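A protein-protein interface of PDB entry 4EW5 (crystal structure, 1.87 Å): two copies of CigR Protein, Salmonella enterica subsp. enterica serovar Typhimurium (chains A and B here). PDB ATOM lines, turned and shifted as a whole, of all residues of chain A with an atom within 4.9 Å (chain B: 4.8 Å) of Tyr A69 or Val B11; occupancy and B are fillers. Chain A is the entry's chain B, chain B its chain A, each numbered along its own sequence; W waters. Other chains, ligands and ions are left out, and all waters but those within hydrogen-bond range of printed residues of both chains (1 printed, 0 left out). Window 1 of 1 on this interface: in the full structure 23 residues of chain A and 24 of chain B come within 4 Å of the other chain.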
ATOM      1  N   SER A  16       3.694  12.952  23.148  1.00  0.00           N
ATOM      2  CA  SER A  16       3.472  14.030  22.187  1.00  0.00           C
ATOM      3  C   SER A  16       2.427  13.675  21.161  1.00  0.00           C
ATOM      4  O   SER A  16       1.587  14.510  20.812  1.00  0.00           O
ATOM      5  CB  SER A  16       4.781  14.410  21.463  1.00  0.00           C
ATOM      6  OG  SER A  16       5.749  14.803  22.370  1.00  0.00           O
ATOM      7  N   PRO A  67       3.797  24.231  21.981  1.00  0.00           N
ATOM      8  CA  PRO A  67       4.977  25.104  22.229  1.00  0.00           C
ATOM      9  C   PRO A  67       5.288  26.046  21.099  1.00  0.00           C
ATOM     10  O   PRO A  67       5.056  25.741  19.897  1.00  0.00           O
ATOM     11  CB  PRO A  67       6.134  24.126  22.430  1.00  0.00           C
ATOM     12  CG  PRO A  67       5.592  22.756  22.233  1.00  0.00           C
ATOM     13  CD  PRO A  67       4.164  22.824  21.741  1.00  0.00           C
ATOM     14  N   TYR A  68       5.848  27.204  21.440  1.00  0.00           N
ATOM     15  CA  TYR A  68       6.301  28.149  20.426  1.00  0.00           C
ATOM     16  C   TYR A  68       7.836  28.233  20.372  1.00  0.00           C
ATOM     17  O   TYR A  68       8.501  28.412  21.379  1.00  0.00           O
ATOM     18  CB  TYR A  68       5.760  29.527  20.733  1.00  0.00           C
ATOM     19  CG  TYR A  68       6.342  30.662  19.921  1.00  0.00           C
ATOM     20  CD1 TYR A  68       5.958  30.856  18.603  1.00  0.00           C
ATOM     21  CD2 TYR A  68       7.246  31.578  20.489  1.00  0.00           C
ATOM     22  CE1 TYR A  68       6.498  31.887  17.833  1.00  0.00           C
ATOM     23  CE2 TYR A  68       7.747  32.666  19.741  1.00  0.00           C
ATOM     24  CZ  TYR A  68       7.336  32.814  18.427  1.00  0.00           C
ATOM     25  OH  TYR A  68       7.815  33.799  17.622  1.00  0.00           O
ATOM     26  N   TYR A  69       8.368  28.171  19.177  1.00  0.00           N
ATOM     27  CA  TYR A  69       9.803  28.269  18.975  1.00  0.00           C
ATOM     28  C   TYR A  69      10.068  29.378  17.943  1.00  0.00           C
ATOM     29  O   TYR A  69       9.766  29.256  16.754  1.00  0.00           O
ATOM     30  CB  TYR A  69      10.343  26.968  18.399  1.00  0.00           C
ATOM     31  CG  TYR A  69      10.058  25.779  19.290  1.00  0.00           C
ATOM     32  CD1 TYR A  69      10.785  25.589  20.458  1.00  0.00           C
ATOM     33  CD2 TYR A  69       8.995  24.912  18.998  1.00  0.00           C
ATOM     34  CE1 TYR A  69      10.533  24.529  21.309  1.00  0.00           C
ATOM     35  CE2 TYR A  69       8.739  23.831  19.815  1.00  0.00           C
ATOM     36  CZ  TYR A  69       9.506  23.652  20.971  1.00  0.00           C
ATOM     37  OH  TYR A  69       9.203  22.647  21.799  1.00  0.00           O
ATOM     38  N   PRO A  70      10.678  30.480  18.390  1.00  0.00           N
ATOM     39  CA  PRO A  70      10.852  31.615  17.487  1.00  0.00           C
ATOM     40  C   PRO A  70      11.569  31.214  16.243  1.00  0.00           C
ATOM     41  O   PRO A  70      12.616  30.524  16.354  1.00  0.00           O
ATOM     42  CB  PRO A  70      11.708  32.580  18.305  1.00  0.00           C
ATOM     43  CG  PRO A  70      11.453  32.180  19.727  1.00  0.00           C
ATOM     44  CD  PRO A  70      11.197  30.715  19.731  1.00  0.00           C
ATOM     45  N   GLY A  71      11.043  31.640  15.078  1.00  0.00           N
ATOM     46  CA  GLY A  71      11.638  31.281  13.793  1.00  0.00           C
ATOM     47  C   GLY A  71      11.153  29.952  13.190  1.00  0.00           C
ATOM     48  O   GLY A  71      11.554  29.584  12.107  1.00  0.00           O
ATOM     49  N   TYR A  72      10.197  29.311  13.855  1.00  0.00           N
ATOM     50  CA  TYR A  72       9.636  28.030  13.410  1.00  0.00           C
ATOM     51  C   TYR A  72       8.131  28.123  13.572  1.00  0.00           C
ATOM     52  O   TYR A  72       7.636  28.896  14.393  1.00  0.00           O
ATOM     53  CB  TYR A  72      10.091  26.879  14.316  1.00  0.00           C
ATOM     54  CG  TYR A  72      11.574  26.659  14.344  1.00  0.00           C
ATOM     55  CD1 TYR A  72      12.371  27.351  15.215  1.00  0.00           C
ATOM     56  CD2 TYR A  72      12.152  25.745  13.517  1.00  0.00           C
ATOM     57  CE1 TYR A  72      13.779  27.178  15.226  1.00  0.00           C
ATOM     58  CE2 TYR A  72      13.554  25.552  13.500  1.00  0.00           C
ATOM     59  CZ  TYR A  72      14.359  26.296  14.346  1.00  0.00           C
ATOM     60  OH  TYR A  72      15.713  26.045  14.406  1.00  0.00           O
ATOM     61  N   TRP A  74       4.388  25.400  13.430  1.00  0.00           N
ATOM     62  CA  TRP A  74       3.680  24.202  13.200  1.00  0.00           C
ATOM     63  C   TRP A  74       2.779  24.361  12.005  1.00  0.00           C
ATOM     64  O   TRP A  74       2.110  25.405  11.848  1.00  0.00           O
ATOM     65  CB  TRP A  74       2.849  23.896  14.430  1.00  0.00           C
ATOM     66  CG  TRP A  74       3.629  23.567  15.659  1.00  0.00           C
ATOM     67  CD1 TRP A  74       3.885  24.391  16.749  1.00  0.00           C
ATOM     68  CD2 TRP A  74       4.255  22.279  16.012  1.00  0.00           C
ATOM     69  NE1 TRP A  74       4.639  23.718  17.683  1.00  0.00           N
ATOM     70  CE2 TRP A  74       4.907  22.477  17.292  1.00  0.00           C
ATOM     71  CE3 TRP A  74       4.403  21.067  15.363  1.00  0.00           C
ATOM     72  CZ2 TRP A  74       5.625  21.478  17.915  1.00  0.00           C
ATOM     73  CZ3 TRP A  74       5.109  20.032  16.016  1.00  0.00           C
ATOM     74  CH2 TRP A  74       5.725  20.243  17.251  1.00  0.00           C
ATOM     75  N   LEU A  83       6.608  20.741  12.632  1.00  0.00           N
ATOM     76  CA  LEU A  83       7.325  21.959  12.942  1.00  0.00           C
ATOM     77  C   LEU A  83       8.320  22.201  11.847  1.00  0.00           C
ATOM     78  O   LEU A  83       9.167  21.379  11.627  1.00  0.00           O
ATOM     79  CB  LEU A  83       8.012  21.824  14.298  1.00  0.00           C
ATOM     80  CG  LEU A  83       8.619  23.140  14.875  1.00  0.00           C
ATOM     81  CD1 LEU A  83       7.520  24.149  15.216  1.00  0.00           C
ATOM     82  CD2 LEU A  83       9.530  22.877  16.052  1.00  0.00           C
ATOM     83  N   ALA A  93      10.478  18.963  13.399  1.00  0.00           N
ATOM     84  CA  ALA A  93       9.906  17.833  14.129  1.00  0.00           C
ATOM     85  C   ALA A  93       8.680  17.374  13.392  1.00  0.00           C
ATOM     86  O   ALA A  93       7.983  18.172  12.765  1.00  0.00           O
ATOM     87  CB  ALA A  93       9.490  18.209  15.542  1.00  0.00           C
ATOM     88  N   GLY B   5       9.650  28.108  23.812  1.00  0.00           N
ATOM     89  CA  GLY B   5      10.490  26.936  24.098  1.00  0.00           C
ATOM     90  C   GLY B   5      11.936  27.172  23.614  1.00  0.00           C
ATOM     91  O   GLY B   5      12.758  26.288  23.675  1.00  0.00           O
ATOM     92  N   GLY B   6      12.225  28.360  23.132  1.00  0.00           N
ATOM     93  CA  GLY B   6      13.566  28.701  22.642  1.00  0.00           C
ATOM     94  C   GLY B   6      13.925  27.895  21.398  1.00  0.00           C
ATOM     95  O   GLY B   6      13.225  27.941  20.390  1.00  0.00           O
ATOM     96  N   LYS B   7      15.037  27.199  21.468  1.00  0.00           N
ATOM     97  CA  LYS B   7      15.482  26.356  20.349  1.00  0.00           C
ATOM     98  C   LYS B   7      14.711  25.058  20.410  1.00  0.00           C
ATOM     99  O   LYS B   7      14.581  24.499  21.462  1.00  0.00           O
ATOM    100  CB  LYS B   7      16.983  26.046  20.431  1.00  0.00           C
ATOM    101  CG  LYS B   7      17.839  27.219  19.992  1.00  0.00           C
ATOM    102  CD  LYS B   7      19.298  26.838  19.686  1.00  0.00           C
ATOM    103  CE  LYS B   7      20.153  26.642  20.953  1.00  0.00           C
ATOM    104  NZ  LYS B   7      21.512  27.280  20.785  1.00  0.00           N
ATOM    105  N   PRO B   8      14.233  24.570  19.263  1.00  0.00           N
ATOM    106  CA  PRO B   8      13.448  23.313  19.253  1.00  0.00           C
ATOM    107  C   PRO B   8      14.389  22.129  19.259  1.00  0.00           C
ATOM    108  O   PRO B   8      14.316  21.309  18.360  1.00  0.00           O
ATOM    109  CB  PRO B   8      12.663  23.383  17.946  1.00  0.00           C
ATOM    110  CG  PRO B   8      13.519  24.261  17.042  1.00  0.00           C
ATOM    111  CD  PRO B   8      14.254  25.228  17.960  1.00  0.00           C
ATOM    112  N   ASP B   9      15.271  22.037  20.251  1.00  0.00           N
ATOM    113  CA  ASP B   9      16.180  20.883  20.346  1.00  0.00           C
ATOM    114  C   ASP B   9      15.640  19.696  21.115  1.00  0.00           C
ATOM    115  O   ASP B   9      16.221  18.629  21.065  1.00  0.00           O
ATOM    116  CB  ASP B   9      17.595  21.279  20.836  1.00  0.00           C
ATOM    117  CG  ASP B   9      17.572  22.210  22.008  1.00  0.00           C
ATOM    118  OD1 ASP B   9      16.518  22.269  22.668  1.00  0.00           O
ATOM    119  OD2 ASP B   9      18.604  22.903  22.242  1.00  0.00           O
ATOM    120  N   HIS B  10      14.510  19.821  21.800  1.00  0.00           N
ATOM    121  CA  HIS B  10      13.859  18.668  22.404  1.00  0.00           C
ATOM    122  C   HIS B  10      12.413  18.912  22.446  1.00  0.00           C
ATOM    123  O   HIS B  10      11.838  19.119  23.518  1.00  0.00           O
ATOM    124  CB  HIS B  10      14.382  18.303  23.800  1.00  0.00           C
ATOM    125  CG  HIS B  10      14.774  19.476  24.646  1.00  0.00           C
ATOM    126  ND1 HIS B  10      13.885  20.457  25.014  1.00  0.00           N
ATOM    127  CD2 HIS B  10      16.021  19.841  25.194  1.00  0.00           C
ATOM    128  CE1 HIS B  10      14.538  21.407  25.748  1.00  0.00           C
ATOM    129  NE2 HIS B  10      15.845  21.017  25.871  1.00  0.00           N
ATOM    130  N   VAL B  11      11.820  18.905  21.271  1.00  0.00           N
ATOM    131  CA  VAL B  11      10.423  19.338  21.175  1.00  0.00           C
ATOM    132  C   VAL B  11       9.493  18.330  21.896  1.00  0.00           C
ATOM    133  O   VAL B  11       8.532  18.688  22.617  1.00  0.00           O
ATOM    134  CB  VAL B  11      10.045  19.438  19.680  1.00  0.00           C
ATOM    135  CG1 VAL B  11       8.514  19.528  19.537  1.00  0.00           C
ATOM    136  CG2 VAL B  11      10.818  20.579  18.963  1.00  0.00           C
ATOM    137  N   GLU B  12       9.754  17.051  21.716  1.00  0.00           N
ATOM    138  CA  GLU B  12       8.898  16.059  22.358  1.00  0.00           C
ATOM    139  C   GLU B  12       9.020  16.118  23.892  1.00  0.00           C
ATOM    140  O   GLU B  12       8.055  15.900  24.618  1.00  0.00           O
ATOM    141  CB  GLU B  12       9.186  14.672  21.794  1.00  0.00           C
ATOM    142  CG  GLU B  12       8.937  14.552  20.311  1.00  0.00           C
ATOM    143  CD  GLU B  12      10.153  15.021  19.420  1.00  0.00           C
ATOM    144  OE1 GLU B  12      11.308  15.389  19.931  1.00  0.00           O
ATOM    145  OE2 GLU B  12       9.951  15.020  18.169  1.00  0.00           O
ATOM    146  N   SER B  13      10.211  16.424  24.406  1.00  0.00           N
ATOM    147  CA  SER B  13      10.357  16.586  25.856  1.00  0.00           C
ATOM    148  C   SER B  13       9.565  17.806  26.321  1.00  0.00           C
ATOM    149  O   SER B  13       8.951  17.731  27.368  1.00  0.00           O
ATOM    150  CB  SER B  13      11.833  16.685  26.258  1.00  0.00           C
ATOM    151  OG  SER B  13      12.502  15.472  25.980  1.00  0.00           O
ATOM    152  N   ASP B  14       9.549  18.903  25.549  1.00  0.00           N
ATOM    153  CA  ASP B  14       8.791  20.105  25.909  1.00  0.00           C
ATOM    154  C   ASP B  14       7.275  19.748  25.973  1.00  0.00           C
ATOM    155  O   ASP B  14       6.559  20.122  26.872  1.00  0.00           O
ATOM    156  CB  ASP B  14       8.975  21.242  24.944  1.00  0.00           C
ATOM    157  CG  ASP B  14      10.403  21.776  24.911  1.00  0.00           C
ATOM    158  OD1 ASP B  14      11.186  21.453  25.811  1.00  0.00           O
ATOM    159  OD2 ASP B  14      10.766  22.374  23.905  1.00  0.00           O
ATOM    160  N   ILE B  15       6.803  19.105  24.928  1.00  0.00           N
ATOM    161  CA  ILE B  15       5.382  18.702  24.898  1.00  0.00           C
ATOM    162  C   ILE B  15       5.003  17.826  26.089  1.00  0.00           C
ATOM    163  O   ILE B  15       3.952  18.027  26.711  1.00  0.00           O
ATOM    164  CB  ILE B  15       5.003  18.064  23.556  1.00  0.00           C
ATOM    165  CG1 ILE B  15       5.157  19.086  22.464  1.00  0.00           C
ATOM    166  CG2 ILE B  15       3.547  17.545  23.592  1.00  0.00           C
ATOM    167  CD1 ILE B  15       5.068  18.579  20.993  1.00  0.00           C
HETATM  168  O   HOH W   1      14.051  29.506  18.252  1.00  0.00           O
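The backbone NH (N) of Gly B5 lies within hydrogen-bond range of the backbone carbonyl oxygen (O) of Tyr A68, 2.7 Å away.
OG of Ser A16 lies close to O of Glu B12 (3.4 Å).
The side-chain carboxylate of Asp B14 sits at hydrogen-bond distance from the side-chain hydroxyl of Tyr A69.
A ring nitrogen (ND1) of His B10 lies within hydrogen-bond range of the side-chain carboxylate (OD1) of Asp B14.
The indole nitrogen (NE1) of Trp A74 is in hydrogen-bond range of the backbone carbonyl oxygen (O) of Pro A67 (3.0 Å).
N of Leu A83 sits at hydrogen-bond distance from O of Ala A93 (2.9 Å).
Pro A67 touches Ile B15.
Tyr A69 touches Gly B5 (CE1 to CA, 3.7 Å).
O of Gly B6 touches CD1 of Tyr A69, at 3.4 Å.
C of Lys B7 touches CD1 of Tyr A69 (3.96 Å).
CA of Pro B8 touches CD1 of Tyr A69, at 3.7 Å.
Val B11 touches Tyr A69.
Pro A70 touches Gly B6 (CD to O, 3.5 Å).
CD of Pro B8 touches CE1 of Tyr A72 (3.4 Å).
Val B11 touches Trp A74 (CG1 to CH2, 3.7 Å).
CG2 of Val B11 touches CD2 of Leu A83, 3.9 Å away.
Of chain B, only Gly B5, Gly B6, Lys B7, Pro B8, Val B11 and Asp B14 come within 4 Å of Tyr A69.
Of the printed residues of chain B, Pro A70 touches Gly B6 (3.5 Å).
Printed residues of chain A within 4 Å of Lys B7: Tyr A69 (3.96 Å).
Of the printed residues of chain A, Val B11 touches Tyr A69, Trp A74 and Leu A83.
Printed residues of chain A within 4 Å of Asp B14: Tyr A69.
The nearest residue of chain A that does not touch Val B11 is Ala A93 (4.3 Å).
Of the 11 printed residues of chain B, 8 touch a printed residue of chain A.
Printed residues of chain B that touch a printed residue of chain A: Gly B5, Gly B6, Lys B7, Pro B8, Val B11, Glu B12, Asp B14 and Ile B15.
Hydrophobic or aromatic side chains of chain B within 4 Å of the printed part of chain A: Pro B8, Val B11 and Ile B15.
Of the 10 printed residues of chain A, 8 touch a printed residue of chain B.
Hydrophobic or aromatic side chains of chain A that line the printed part of chain B: Pro A67, Tyr A69, Pro A70, Tyr A72, Trp A74 and Leu A83.
Among the printed residues, 15 pairs touch across the chains.
Among the printed residues, no Asp or Glu carboxylate lies within 4 Å of a Lys or Arg side-chain nitrogen of the other chain.
No position is printed for both chains.
Of the 15 pairs that touch across the chains among the printed residues, none has its exchanged pair printed and touching as well.
Water W1 bridges the backbone carbonyl oxygen of Pro A70 (2.6 Å) and the backbone carbonyl oxygen of Gly B6 (2.8 Å).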
